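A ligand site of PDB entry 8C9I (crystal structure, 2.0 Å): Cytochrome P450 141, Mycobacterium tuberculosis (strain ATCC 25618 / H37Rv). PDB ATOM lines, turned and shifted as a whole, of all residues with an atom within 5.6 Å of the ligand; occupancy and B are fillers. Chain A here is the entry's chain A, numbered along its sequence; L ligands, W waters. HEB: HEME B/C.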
ATOM      1  N   LEU A  56      -6.820  -3.168  14.682  1.00  0.00           N
ATOM      2  CA  LEU A  56      -7.410  -4.401  14.157  1.00  0.00           C
ATOM      3  C   LEU A  56      -7.338  -5.548  15.160  1.00  0.00           C
ATOM      4  O   LEU A  56      -8.155  -6.481  15.071  1.00  0.00           O
ATOM      5  CB  LEU A  56      -6.697  -4.805  12.860  1.00  0.00           C
ATOM      6  CG  LEU A  56      -6.950  -3.909  11.655  1.00  0.00           C
ATOM      7  CD1 LEU A  56      -6.049  -4.296  10.493  1.00  0.00           C
ATOM      8  CD2 LEU A  56      -8.420  -3.965  11.234  1.00  0.00           C
ATOM      9  N   LEU A  84     -19.272 -12.385   8.423  1.00  0.00           N
ATOM     10  CA  LEU A  84     -18.090 -12.526   9.275  1.00  0.00           C
ATOM     11  C   LEU A  84     -17.578 -11.173   9.721  1.00  0.00           C
ATOM     12  O   LEU A  84     -16.946 -11.065  10.776  1.00  0.00           O
ATOM     13  CB  LEU A  84     -16.994 -13.297   8.537  1.00  0.00           C
ATOM     14  CG  LEU A  84     -17.259 -14.776   8.252  1.00  0.00           C
ATOM     15  CD1 LEU A  84     -16.051 -15.397   7.562  1.00  0.00           C
ATOM     16  CD2 LEU A  84     -17.584 -15.544   9.524  1.00  0.00           C
ATOM     17  N   LEU A  85     -17.839 -10.124   8.938  1.00  0.00           N
ATOM     18  CA  LEU A  85     -17.492  -8.766   9.315  1.00  0.00           C
ATOM     19  C   LEU A  85     -18.617  -8.071  10.074  1.00  0.00           C
ATOM     20  O   LEU A  85     -18.621  -6.843  10.179  1.00  0.00           O
ATOM     21  CB  LEU A  85     -17.128  -7.965   8.063  1.00  0.00           C
ATOM     22  CG  LEU A  85     -15.788  -8.358   7.433  1.00  0.00           C
ATOM     23  CD1 LEU A  85     -15.805  -8.137   5.934  1.00  0.00           C
ATOM     24  CD2 LEU A  85     -14.638  -7.608   8.083  1.00  0.00           C
ATOM     25  N   HIS A  92     -17.730 -15.507  16.197  1.00  0.00           N
ATOM     26  CA  HIS A  92     -16.845 -15.328  15.054  1.00  0.00           C
ATOM     27  C   HIS A  92     -15.786 -16.421  15.017  1.00  0.00           C
ATOM     28  O   HIS A  92     -15.485 -16.966  13.943  1.00  0.00           O
ATOM     29  CB  HIS A  92     -16.194 -13.950  15.123  1.00  0.00           C
ATOM     30  CG  HIS A  92     -15.226 -13.683  14.005  1.00  0.00           C
ATOM     31  ND1 HIS A  92     -13.864 -13.744  14.187  1.00  0.00           N
ATOM     32  CD2 HIS A  92     -15.424 -13.363  12.706  1.00  0.00           C
ATOM     33  CE1 HIS A  92     -13.260 -13.469  13.044  1.00  0.00           C
ATOM     34  NE2 HIS A  92     -14.187 -13.224  12.130  1.00  0.00           N
ATOM     35  N   ARG A  96     -15.007 -19.107  11.910  1.00  0.00           N
ATOM     36  CA  ARG A  96     -13.706 -19.172  11.261  1.00  0.00           C
ATOM     37  C   ARG A  96     -13.100 -20.569  11.352  1.00  0.00           C
ATOM     38  O   ARG A  96     -12.417 -21.011  10.418  1.00  0.00           O
ATOM     39  CB  ARG A  96     -12.762 -18.136  11.868  1.00  0.00           C
ATOM     40  CG  ARG A  96     -13.139 -16.699  11.539  1.00  0.00           C
ATOM     41  CD  ARG A  96     -12.935 -16.395  10.060  1.00  0.00           C
ATOM     42  NE  ARG A  96     -11.545 -16.596   9.670  1.00  0.00           N
ATOM     43  CZ  ARG A  96     -10.671 -15.617   9.425  1.00  0.00           C
ATOM     44  NH1 ARG A  96     -11.028 -14.343   9.474  1.00  0.00           N
ATOM     45  NH2 ARG A  96      -9.420 -15.928   9.126  1.00  0.00           N
ATOM     46  N   LEU A  99     -14.726 -22.523   8.516  1.00  0.00           N
ATOM     47  CA  LEU A  99     -14.143 -22.104   7.250  1.00  0.00           C
ATOM     48  C   LEU A  99     -12.713 -22.605   7.113  1.00  0.00           C
ATOM     49  O   LEU A  99     -12.308 -23.061   6.030  1.00  0.00           O
ATOM     50  CB  LEU A  99     -14.199 -20.582   7.127  1.00  0.00           C
ATOM     51  CG  LEU A  99     -13.671 -19.966   5.830  1.00  0.00           C
ATOM     52  CD1 LEU A  99     -14.364 -20.564   4.617  1.00  0.00           C
ATOM     53  CD2 LEU A  99     -13.859 -18.451   5.857  1.00  0.00           C
ATOM     54  N   MET A 148     -14.300 -18.846  -7.977  1.00  0.00           N
ATOM     55  CA  MET A 148     -15.390 -18.894  -7.005  1.00  0.00           C
ATOM     56  C   MET A 148     -16.377 -20.004  -7.362  1.00  0.00           C
ATOM     57  O   MET A 148     -16.930 -20.657  -6.482  1.00  0.00           O
ATOM     58  CB  MET A 148     -16.089 -17.545  -6.949  1.00  0.00           C
ATOM     59  CG  MET A 148     -17.304 -17.513  -6.025  1.00  0.00           C
ATOM     60  SD  MET A 148     -16.887 -17.743  -4.290  1.00  0.00           S
ATOM     61  CE  MET A 148     -15.657 -16.469  -4.019  1.00  0.00           C
ATOM     62  N   LEU A 151     -15.160 -23.065  -5.798  1.00  0.00           N
ATOM     63  CA  LEU A 151     -15.356 -23.076  -4.356  1.00  0.00           C
ATOM     64  C   LEU A 151     -16.806 -23.390  -4.001  1.00  0.00           C
ATOM     65  O   LEU A 151     -17.069 -24.135  -3.043  1.00  0.00           O
ATOM     66  CB  LEU A 151     -14.944 -21.742  -3.747  1.00  0.00           C
ATOM     67  CG  LEU A 151     -13.497 -21.276  -3.952  1.00  0.00           C
ATOM     68  CD1 LEU A 151     -13.226 -20.045  -3.121  1.00  0.00           C
ATOM     69  CD2 LEU A 151     -12.524 -22.387  -3.604  1.00  0.00           C
ATOM     70  N   MET A 228     -22.051 -16.203   6.477  1.00  0.00           N
ATOM     71  CA  MET A 228     -20.641 -16.472   6.198  1.00  0.00           C
ATOM     72  C   MET A 228     -20.418 -16.658   4.701  1.00  0.00           C
ATOM     73  O   MET A 228     -19.481 -16.090   4.130  1.00  0.00           O
ATOM     74  CB  MET A 228     -20.178 -17.715   6.954  1.00  0.00           C
ATOM     75  CG  MET A 228     -18.747 -18.132   6.629  1.00  0.00           C
ATOM     76  SD  MET A 228     -18.046 -19.250   7.855  1.00  0.00           S
ATOM     77  CE  MET A 228     -18.702 -20.819   7.287  1.00  0.00           C
ATOM     78  N   THR A 231     -20.331 -13.461   2.893  1.00  0.00           N
ATOM     79  CA  THR A 231     -19.048 -12.792   3.048  1.00  0.00           C
ATOM     80  C   THR A 231     -18.007 -13.366   2.088  1.00  0.00           C
ATOM     81  O   THR A 231     -17.247 -12.619   1.471  1.00  0.00           O
ATOM     82  CB  THR A 231     -18.544 -12.907   4.487  1.00  0.00           C
ATOM     83  OG1 THR A 231     -19.630 -12.747   5.404  1.00  0.00           O
ATOM     84  CG2 THR A 231     -17.485 -11.851   4.773  1.00  0.00           C
ATOM     85  N   VAL A 232     -17.972 -14.698   1.958  1.00  0.00           N
ATOM     86  CA  VAL A 232     -17.019 -15.329   1.061  1.00  0.00           C
ATOM     87  C   VAL A 232     -17.253 -14.870  -0.370  1.00  0.00           C
ATOM     88  O   VAL A 232     -16.308 -14.566  -1.110  1.00  0.00           O
ATOM     89  CB  VAL A 232     -17.115 -16.859   1.178  1.00  0.00           C
ATOM     90  CG1 VAL A 232     -16.317 -17.541   0.071  1.00  0.00           C
ATOM     91  CG2 VAL A 232     -16.648 -17.319   2.551  1.00  0.00           C
ATOM     92  N   GLY A 235     -16.389 -11.010  -0.803  1.00  0.00           N
ATOM     93  CA  GLY A 235     -14.970 -10.750  -0.670  1.00  0.00           C
ATOM     94  C   GLY A 235     -14.067 -11.579  -1.559  1.00  0.00           C
ATOM     95  O   GLY A 235     -12.884 -11.252  -1.694  1.00  0.00           O
ATOM     96  N   GLY A 236     -14.590 -12.644  -2.162  1.00  0.00           N
ATOM     97  CA  GLY A 236     -13.783 -13.560  -2.942  1.00  0.00           C
ATOM     98  C   GLY A 236     -13.850 -13.409  -4.430  1.00  0.00           C
ATOM     99  O   GLY A 236     -13.139 -14.120  -5.144  1.00  0.00           O
ATOM    100  N   THR A 239     -12.356  -8.800  -5.125  1.00  0.00           N
ATOM    101  CA  THR A 239     -11.032  -8.478  -4.588  1.00  0.00           C
ATOM    102  C   THR A 239      -9.920  -9.129  -5.401  1.00  0.00           C
ATOM    103  O   THR A 239      -8.992  -8.411  -5.812  1.00  0.00           O
ATOM    104  CB  THR A 239     -10.960  -8.860  -3.107  1.00  0.00           C
ATOM    105  OG1 THR A 239     -11.778  -7.967  -2.340  1.00  0.00           O
ATOM    106  CG2 THR A 239      -9.522  -8.783  -2.590  1.00  0.00           C
ATOM    107  N   PRO A 240      -9.931 -10.441  -5.657  1.00  0.00           N
ATOM    108  CA  PRO A 240      -8.881 -11.000  -6.525  1.00  0.00           C
ATOM    109  C   PRO A 240      -8.847 -10.350  -7.903  1.00  0.00           C
ATOM    110  O   PRO A 240      -7.764 -10.107  -8.452  1.00  0.00           O
ATOM    111  CB  PRO A 240      -9.242 -12.490  -6.618  1.00  0.00           C
ATOM    112  CG  PRO A 240     -10.180 -12.749  -5.493  1.00  0.00           C
ATOM    113  CD  PRO A 240     -10.870 -11.466  -5.178  1.00  0.00           C
ATOM    114  N   VAL A 243      -7.118  -6.878  -7.570  1.00  0.00           N
ATOM    115  CA  VAL A 243      -5.687  -6.946  -7.303  1.00  0.00           C
ATOM    116  C   VAL A 243      -4.943  -7.420  -8.543  1.00  0.00           C
ATOM    117  O   VAL A 243      -3.883  -6.876  -8.897  1.00  0.00           O
ATOM    118  CB  VAL A 243      -5.406  -7.854  -6.098  1.00  0.00           C
ATOM    119  CG1 VAL A 243      -3.901  -8.017  -5.888  1.00  0.00           C
ATOM    120  CG2 VAL A 243      -6.050  -7.285  -4.843  1.00  0.00           C
ATOM    121  N   VAL A 276       0.415  -7.407  -3.643  1.00  0.00           N
ATOM    122  CA  VAL A 276      -0.677  -7.209  -2.694  1.00  0.00           C
ATOM    123  C   VAL A 276      -0.386  -6.023  -1.782  1.00  0.00           C
ATOM    124  O   VAL A 276      -1.307  -5.305  -1.387  1.00  0.00           O
ATOM    125  CB  VAL A 276      -0.957  -8.504  -1.898  1.00  0.00           C
ATOM    126  CG1 VAL A 276      -1.431  -9.601  -2.828  1.00  0.00           C
ATOM    127  CG2 VAL A 276       0.271  -8.942  -1.108  1.00  0.00           C
ATOM    128  N   GLU A 285     -10.689  -0.067   5.382  1.00  0.00           N
ATOM    129  CA  GLU A 285     -11.260  -1.350   5.755  1.00  0.00           C
ATOM    130  C   GLU A 285     -12.728  -1.195   6.134  1.00  0.00           C
ATOM    131  O   GLU A 285     -13.306  -0.101   6.088  1.00  0.00           O
ATOM    132  CB  GLU A 285     -10.463  -1.981   6.896  1.00  0.00           C
ATOM    133  CG  GLU A 285      -9.392  -2.949   6.428  1.00  0.00           C
ATOM    134  CD  GLU A 285      -8.436  -2.307   5.440  1.00  0.00           C
ATOM    135  OE1 GLU A 285      -8.442  -2.699   4.250  1.00  0.00           O
ATOM    136  OE2 GLU A 285      -7.686  -1.400   5.851  1.00  0.00           O
ATOM    137  N   HIS A 286     -13.356  -2.308   6.526  1.00  0.00           N
ATOM    138  CA  HIS A 286     -14.740  -2.269   6.953  1.00  0.00           C
ATOM    139  C   HIS A 286     -14.866  -1.545   8.287  1.00  0.00           C
ATOM    140  O   HIS A 286     -13.924  -1.452   9.074  1.00  0.00           O
ATOM    141  CB  HIS A 286     -15.301  -3.689   7.065  1.00  0.00           C
ATOM    142  CG  HIS A 286     -15.299  -4.437   5.762  1.00  0.00           C
ATOM    143  ND1 HIS A 286     -14.218  -5.148   5.306  1.00  0.00           N
ATOM    144  CD2 HIS A 286     -16.257  -4.558   4.803  1.00  0.00           C
ATOM    145  CE1 HIS A 286     -14.504  -5.689   4.139  1.00  0.00           C
ATOM    146  NE2 HIS A 286     -15.739  -5.347   3.815  1.00  0.00           N
ATOM    147  N   ARG A 288     -15.535  -0.286  11.978  1.00  0.00           N
ATOM    148  CA  ARG A 288     -15.537  -0.745  13.360  1.00  0.00           C
ATOM    149  C   ARG A 288     -16.144   0.356  14.225  1.00  0.00           C
ATOM    150  O   ARG A 288     -16.099   1.534  13.879  1.00  0.00           O
ATOM    151  CB  ARG A 288     -14.124  -1.078  13.858  1.00  0.00           C
ATOM    152  CG  ARG A 288     -13.724  -2.524  13.663  1.00  0.00           C
ATOM    153  CD  ARG A 288     -13.409  -2.831  12.206  1.00  0.00           C
ATOM    154  NE  ARG A 288     -12.584  -4.012  12.057  1.00  0.00           N
ATOM    155  CZ  ARG A 288     -12.179  -4.501  10.893  1.00  0.00           C
ATOM    156  NH1 ARG A 288     -12.509  -3.925   9.751  1.00  0.00           N
ATOM    157  NH2 ARG A 288     -11.412  -5.588  10.870  1.00  0.00           N
ATOM    158  N   ILE A 311      -5.423  -0.246   5.649  1.00  0.00           N
ATOM    159  CA  ILE A 311      -4.306  -1.116   5.296  1.00  0.00           C
ATOM    160  C   ILE A 311      -3.565  -0.534   4.097  1.00  0.00           C
ATOM    161  O   ILE A 311      -2.340  -0.662   3.991  1.00  0.00           O
ATOM    162  CB  ILE A 311      -4.808  -2.537   5.014  1.00  0.00           C
ATOM    163  CG1 ILE A 311      -5.101  -3.256   6.330  1.00  0.00           C
ATOM    164  CG2 ILE A 311      -3.799  -3.316   4.187  1.00  0.00           C
ATOM    165  CD1 ILE A 311      -5.959  -4.494   6.186  1.00  0.00           C
ATOM    166  N   ILE A 337       0.812  -6.057   5.691  1.00  0.00           N
ATOM    167  CA  ILE A 337      -0.419  -6.606   6.254  1.00  0.00           C
ATOM    168  C   ILE A 337      -1.536  -6.518   5.209  1.00  0.00           C
ATOM    169  O   ILE A 337      -2.681  -6.206   5.533  1.00  0.00           O
ATOM    170  CB  ILE A 337      -0.826  -5.877   7.549  1.00  0.00           C
ATOM    171  CG1 ILE A 337      -0.842  -4.363   7.329  1.00  0.00           C
ATOM    172  CG2 ILE A 337       0.132  -6.240   8.671  1.00  0.00           C
ATOM    173  CD1 ILE A 337      -1.439  -3.587   8.482  1.00  0.00           C
ATOM    174  N   ALA A 338      -1.192  -6.816   3.949  1.00  0.00           N
ATOM    175  CA  ALA A 338      -2.157  -6.703   2.867  1.00  0.00           C
ATOM    176  C   ALA A 338      -3.353  -7.627   3.077  1.00  0.00           C
ATOM    177  O   ALA A 338      -4.450  -7.336   2.579  1.00  0.00           O
ATOM    178  CB  ALA A 338      -1.482  -7.009   1.530  1.00  0.00           C
ATOM    179  N   PHE A 339      -3.168  -8.734   3.776  1.00  0.00           N
ATOM    180  CA  PHE A 339      -4.250  -9.669   4.059  1.00  0.00           C
ATOM    181  C   PHE A 339      -4.906  -9.411   5.404  1.00  0.00           C
ATOM    182  O   PHE A 339      -5.616 -10.279   5.917  1.00  0.00           O
ATOM    183  CB  PHE A 339      -3.739 -11.111   3.975  1.00  0.00           C
ATOM    184  CG  PHE A 339      -3.484 -11.573   2.580  1.00  0.00           C
ATOM    185  CD1 PHE A 339      -4.534 -11.918   1.740  1.00  0.00           C
ATOM    186  CD2 PHE A 339      -2.189 -11.667   2.085  1.00  0.00           C
ATOM    187  CE1 PHE A 339      -4.305 -12.347   0.447  1.00  0.00           C
ATOM    188  CE2 PHE A 339      -1.952 -12.093   0.798  1.00  0.00           C
ATOM    189  CZ  PHE A 339      -3.009 -12.431  -0.033  1.00  0.00           C
ATOM    190  N   GLY A 340      -4.695  -8.238   5.993  1.00  0.00           N
ATOM    191  CA  GLY A 340      -5.363  -7.875   7.220  1.00  0.00           C
ATOM    192  C   GLY A 340      -4.585  -8.289   8.451  1.00  0.00           C
ATOM    193  O   GLY A 340      -3.465  -8.798   8.398  1.00  0.00           O
ATOM    194  N   TYR A 341      -5.218  -8.055   9.600  1.00  0.00           N
ATOM    195  CA  TYR A 341      -4.608  -8.330  10.884  1.00  0.00           C
ATOM    196  C   TYR A 341      -5.714  -8.507  11.915  1.00  0.00           C
ATOM    197  O   TYR A 341      -6.818  -7.970  11.760  1.00  0.00           O
ATOM    198  CB  TYR A 341      -3.651  -7.205  11.300  1.00  0.00           C
ATOM    199  CG  TYR A 341      -2.685  -7.584  12.397  1.00  0.00           C
ATOM    200  CD1 TYR A 341      -1.601  -8.411  12.134  1.00  0.00           C
ATOM    201  CD2 TYR A 341      -2.856  -7.105  13.692  1.00  0.00           C
ATOM    202  CE1 TYR A 341      -0.718  -8.754  13.136  1.00  0.00           C
ATOM    203  CE2 TYR A 341      -1.973  -7.448  14.694  1.00  0.00           C
ATOM    204  CZ  TYR A 341      -0.903  -8.267  14.413  1.00  0.00           C
ATOM    205  OH  TYR A 341      -0.020  -8.610  15.415  1.00  0.00           O
ATOM    206  N   PRO A 343      -8.430 -10.782  14.375  1.00  0.00           N
ATOM    207  CA  PRO A 343      -9.359 -11.906  14.141  1.00  0.00           C
ATOM    208  C   PRO A 343      -9.969 -11.916  12.748  1.00  0.00           C
ATOM    209  O   PRO A 343     -10.277 -13.003  12.236  1.00  0.00           O
ATOM    210  CB  PRO A 343     -10.436 -11.707  15.218  1.00  0.00           C
ATOM    211  CG  PRO A 343      -9.788 -10.862  16.266  1.00  0.00           C
ATOM    212  CD  PRO A 343      -8.801  -9.987  15.567  1.00  0.00           C
ATOM    213  N   HIS A 344     -10.155 -10.754  12.124  1.00  0.00           N
ATOM    214  CA  HIS A 344     -10.810 -10.684  10.824  1.00  0.00           C
ATOM    215  C   HIS A 344      -9.820 -10.765   9.663  1.00  0.00           C
ATOM    216  O   HIS A 344     -10.210 -10.485   8.528  1.00  0.00           O
ATOM    217  CB  HIS A 344     -11.633  -9.400  10.720  1.00  0.00           C
ATOM    218  CG  HIS A 344     -12.790  -9.354  11.682  1.00  0.00           C
ATOM    219  ND1 HIS A 344     -14.008  -9.924  11.403  1.00  0.00           N
ATOM    220  CD2 HIS A 344     -12.904  -8.795  12.913  1.00  0.00           C
ATOM    221  CE1 HIS A 344     -14.831  -9.718  12.424  1.00  0.00           C
ATOM    222  NE2 HIS A 344     -14.183  -9.039  13.351  1.00  0.00           N
ATOM    223  N   ALA A 345      -8.568 -11.135   9.916  1.00  0.00           N
ATOM    224  CA  ALA A 345      -7.604 -11.277   8.840  1.00  0.00           C
ATOM    225  C   ALA A 345      -8.093 -12.318   7.835  1.00  0.00           C
ATOM    226  O   ALA A 345      -8.807 -13.252   8.172  1.00  0.00           O
ATOM    227  CB  ALA A 345      -6.237 -11.674   9.399  1.00  0.00           C
ATOM    228  N   CYS A 346      -7.672 -12.145   6.582  1.00  0.00           N
ATOM    229  CA  CYS A 346      -8.247 -12.907   5.481  1.00  0.00           C
ATOM    230  C   CYS A 346      -8.115 -14.406   5.724  1.00  0.00           C
ATOM    231  O   CYS A 346      -7.012 -14.901   5.975  1.00  0.00           O
ATOM    232  CB  CYS A 346      -7.559 -12.532   4.166  1.00  0.00           C
ATOM    233  SG  CYS A 346      -8.377 -13.221   2.713  1.00  0.00           S
ATOM    234  N   PRO A 347      -9.212 -15.180   5.644  1.00  0.00           N
ATOM    235  CA  PRO A 347      -9.082 -16.633   5.756  1.00  0.00           C
ATOM    236  C   PRO A 347      -8.529 -17.287   4.508  1.00  0.00           C
ATOM    237  O   PRO A 347      -8.073 -18.435   4.576  1.00  0.00           O
ATOM    238  CB  PRO A 347     -10.523 -17.094   6.026  1.00  0.00           C
ATOM    239  CG  PRO A 347     -11.359 -16.080   5.334  1.00  0.00           C
ATOM    240  CD  PRO A 347     -10.609 -14.767   5.428  1.00  0.00           C
ATOM    241  N   ALA A 348      -8.526 -16.588   3.365  1.00  0.00           N
ATOM    242  CA  ALA A 348      -8.096 -17.131   2.092  1.00  0.00           C
ATOM    243  C   ALA A 348      -6.725 -16.624   1.667  1.00  0.00           C
ATOM    244  O   ALA A 348      -6.417 -16.612   0.467  1.00  0.00           O
ATOM    245  CB  ALA A 348      -9.135 -16.811   1.018  1.00  0.00           C
ATOM    246  N   TYR A 351      -4.731 -19.490   0.060  1.00  0.00           N
ATOM    247  CA  TYR A 351      -5.363 -19.774  -1.226  1.00  0.00           C
ATOM    248  C   TYR A 351      -5.092 -18.651  -2.221  1.00  0.00           C
ATOM    249  O   TYR A 351      -4.769 -18.914  -3.387  1.00  0.00           O
ATOM    250  CB  TYR A 351      -6.854 -19.981  -1.004  1.00  0.00           C
ATOM    251  CG  TYR A 351      -7.711 -19.974  -2.247  1.00  0.00           C
ATOM    252  CD1 TYR A 351      -7.790 -21.088  -3.065  1.00  0.00           C
ATOM    253  CD2 TYR A 351      -8.470 -18.855  -2.590  1.00  0.00           C
ATOM    254  CE1 TYR A 351      -8.585 -21.094  -4.193  1.00  0.00           C
ATOM    255  CE2 TYR A 351      -9.255 -18.847  -3.721  1.00  0.00           C
ATOM    256  CZ  TYR A 351      -9.319 -19.968  -4.521  1.00  0.00           C
ATOM    257  OH  TYR A 351     -10.108 -19.963  -5.642  1.00  0.00           O
ATOM    258  N   SER A 352      -5.194 -17.397  -1.784  1.00  0.00           N
ATOM    259  CA  SER A 352      -5.013 -16.271  -2.698  1.00  0.00           C
ATOM    260  C   SER A 352      -3.562 -16.157  -3.160  1.00  0.00           C
ATOM    261  O   SER A 352      -3.302 -15.837  -4.318  1.00  0.00           O
ATOM    262  CB  SER A 352      -5.456 -14.978  -2.015  1.00  0.00           C
ATOM    263  OG  SER A 352      -6.848 -14.983  -1.783  1.00  0.00           O
ATOM    264  N   LEU A 356      -2.574 -16.176  -7.120  1.00  0.00           N
ATOM    265  CA  LEU A 356      -1.889 -15.076  -7.803  1.00  0.00           C
ATOM    266  C   LEU A 356      -0.535 -15.528  -8.336  1.00  0.00           C
ATOM    267  O   LEU A 356      -0.100 -15.074  -9.403  1.00  0.00           O
ATOM    268  CB  LEU A 356      -1.731 -13.897  -6.850  1.00  0.00           C
ATOM    269  CG  LEU A 356      -2.819 -12.831  -6.944  1.00  0.00           C
ATOM    270  CD1 LEU A 356      -4.193 -13.454  -6.828  1.00  0.00           C
ATOM    271  CD2 LEU A 356      -2.625 -11.759  -5.872  1.00  0.00           C
HETATM  272 FE   HEB L   1      -9.910 -11.706   1.896  1.00  0.00          FE
HETATM  273  CHA HEB L   1     -11.057 -10.506   4.955  1.00  0.00           C
HETATM  274  CHB HEB L   1      -7.703  -9.069   1.738  1.00  0.00           C
HETATM  275  CHC HEB L   1      -9.019 -12.651  -1.268  1.00  0.00           C
HETATM  276  CHD HEB L   1     -12.620 -13.823   1.770  1.00  0.00           C
HETATM  277  NA  HEB L   1      -9.476 -10.083   3.126  1.00  0.00           N
HETATM  278  C1A HEB L   1     -10.053  -9.784   4.350  1.00  0.00           C
HETATM  279  C2A HEB L   1      -9.410  -8.596   4.868  1.00  0.00           C
HETATM  280  C3A HEB L   1      -8.489  -8.200   3.977  1.00  0.00           C
HETATM  281  C4A HEB L   1      -8.513  -9.126   2.866  1.00  0.00           C
HETATM  282  CMA HEB L   1      -7.565  -6.971   4.119  1.00  0.00           C
HETATM  283  CAA HEB L   1      -9.727  -7.895   6.205  1.00  0.00           C
HETATM  284  CBA HEB L   1     -10.787  -6.807   6.002  1.00  0.00           C
HETATM  285  CGA HEB L   1     -11.063  -6.110   7.314  1.00  0.00           C
HETATM  286  O1A HEB L   1     -11.899  -5.174   7.335  1.00  0.00           O
HETATM  287  O2A HEB L   1     -10.440  -6.490   8.336  1.00  0.00           O
HETATM  288  NB  HEB L   1      -8.650 -10.945   0.462  1.00  0.00           N
HETATM  289  C1B HEB L   1      -7.732  -9.937   0.666  1.00  0.00           C
HETATM  290  C2B HEB L   1      -6.790  -9.955  -0.445  1.00  0.00           C
HETATM  291  C3B HEB L   1      -7.152 -10.952  -1.269  1.00  0.00           C
HETATM  292  C4B HEB L   1      -8.330 -11.589  -0.714  1.00  0.00           C
HETATM  293  CMB HEB L   1      -5.605  -8.979  -0.586  1.00  0.00           C
HETATM  294  CAB HEB L   1      -6.500 -11.404  -2.603  1.00  0.00           C
HETATM  295  CBB HEB L   1      -5.521 -10.713  -3.196  1.00  0.00           C
HETATM  296  NC  HEB L   1     -10.716 -12.935   0.477  1.00  0.00           N
HETATM  297  C1C HEB L   1     -10.091 -13.296  -0.702  1.00  0.00           C
HETATM  298  C2C HEB L   1     -10.762 -14.472  -1.220  1.00  0.00           C
HETATM  299  C3C HEB L   1     -11.755 -14.792  -0.382  1.00  0.00           C
HETATM  300  C4C HEB L   1     -11.746 -13.836   0.705  1.00  0.00           C
HETATM  301  CMC HEB L   1     -10.369 -15.194  -2.533  1.00  0.00           C
HETATM  302  CAC HEB L   1     -12.773 -15.961  -0.477  1.00  0.00           C
HETATM  303  CBC HEB L   1     -12.623 -16.984  -1.328  1.00  0.00           C
HETATM  304  ND  HEB L   1     -11.551 -12.075   3.136  1.00  0.00           N
HETATM  305  C1D HEB L   1     -12.530 -13.012   2.883  1.00  0.00           C
HETATM  306  C2D HEB L   1     -13.448 -13.000   4.018  1.00  0.00           C
HETATM  307  C3D HEB L   1     -13.020 -12.092   4.889  1.00  0.00           C
HETATM  308  C4D HEB L   1     -11.814 -11.491   4.361  1.00  0.00           C
HETATM  309  CMD HEB L   1     -14.695 -13.900   4.147  1.00  0.00           C
HETATM  310  CAD HEB L   1     -13.677 -11.719   6.244  1.00  0.00           C
HETATM  311  CBD HEB L   1     -13.048 -12.563   7.356  1.00  0.00           C
HETATM  312  CGD HEB L   1     -13.598 -12.152   8.700  1.00  0.00           C
HETATM  313  O1D HEB L   1     -14.211 -11.054   8.801  1.00  0.00           O
HETATM  314  O2D HEB L   1     -13.429 -12.924   9.680  1.00  0.00           O
HETATM  315  O   HOH W   1      -8.207  -7.499   9.298  1.00  0.00           O
HETATM  316  O   HOH W   2     -11.281 -10.572   0.795  1.00  0.00           O
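An iron atom (FE) of the ligand is bound by the side-chain sulfur (SG) of Cys 346, 2.3 Å away.
NE2 of His 92 is in hydrogen-bond range of O2D of the ligand (2.6 Å).
The guanidinium group of Arg 288 lies within salt-bridge range of an oxygen (O1A) of the ligand (2.8 Å).
The guanidinium group of Arg 96 lies within salt-bridge range of an oxygen (O2D) of the ligand (2.8 Å).
An oxygen (O1D) of the ligand is in hydrogen-bond range of a ring nitrogen (ND1) of His 344.
O1A of the ligand is in hydrogen-bond range of N of His 286 (3.3 Å).
A ring nitrogen (ND1) of His 286 lies within hydrogen-bond range of an oxygen (O1A) of the ligand.
SG of Cys 346 lies close to N of Ala 348 (3.4 Å).
A ring nitrogen (NE2) of His 92 sits at hydrogen-bond distance from a ring nitrogen (ND1) of His 344 (3.4 Å).
NH1 of Arg 288 sits at hydrogen-bond distance from O of His 286 (2.9 Å).
NH1 of Arg 96 sits at hydrogen-bond distance from O of Pro 343.
ND1 of His 344 sits close to O of Leu 84 (3.2 Å).
The side-chain hydroxyl (OG) of Ser 352 is in hydrogen-bond range of the backbone carbonyl oxygen (O) of Ala 348.
N of Leu 84 is in hydrogen-bond range of OG1 of Thr 231, at 3.1 Å.
OE2 of Glu 285 sits at hydrogen-bond distance from N of Ile 311.
The backbone carbonyl oxygen (O) of Leu 84 sits close to an oxygen (O1D) of the ligand, 3.4 Å away.
NC of the ligand sits close to O of Gly 235 (3.5 Å).
CG of Leu 85 touches O1D of the ligand, at 3.4 Å.
Leu 151 touches the ligand.
CG2 of Thr 231 touches CMD of the ligand, 3.5 Å away.
Val 232 touches the ligand.
Gly 236 touches the ligand (CA to C3C, 3.5 Å).
CG2 of Thr 239 touches C3B of the ligand (3.5 Å).
CG of Pro 240 touches CMC of the ligand (3.8 Å).
Val 243 touches the ligand.
CG of Glu 285 touches O1A of the ligand, at 3.5 Å.
Ile 311 touches the ligand (CD1 to CMA, 3.6 Å).
Ala 338 touches the ligand (O to CMA, 3.5 Å).
Phe 339 touches the ligand.
Gly 340 touches the ligand (N to CMA, 3.7 Å).
CD of Pro 347 touches C2D of the ligand, 3.6 Å away.
Ala 348 touches the ligand.
Tyr 351 touches the ligand (CE2 to CMC, 3.9996 Å).
OG of Ser 352 touches CHC of the ligand (3.2 Å).
Hydrophobic or aromatic side chains within 4 Å of the ligand: Leu 84, Leu 85, His 92, Leu 151, Val 232, Pro 240, Val 243, His 286, Ile 311, Phe 339, His 344, Pro 347, Ala 348 and Tyr 351.
Within 4 Å of the ligand: Leu 84, Leu 85, His 92, Arg 96, Leu 151, Thr 231, Val 232, Gly 235, Gly 236, Thr 239, Pro 240, Val 243, Glu 285, His 286, Arg 288, Ile 311, Ala 338, Phe 339, Gly 340, His 344, Cys 346, Pro 347, Ala 348, Tyr 351 and Ser 352.
Water W1 lies within hydrogen-bond range of an oxygen (O2A) of the ligand and the backbone carbonyl oxygen (O) of Tyr 341.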
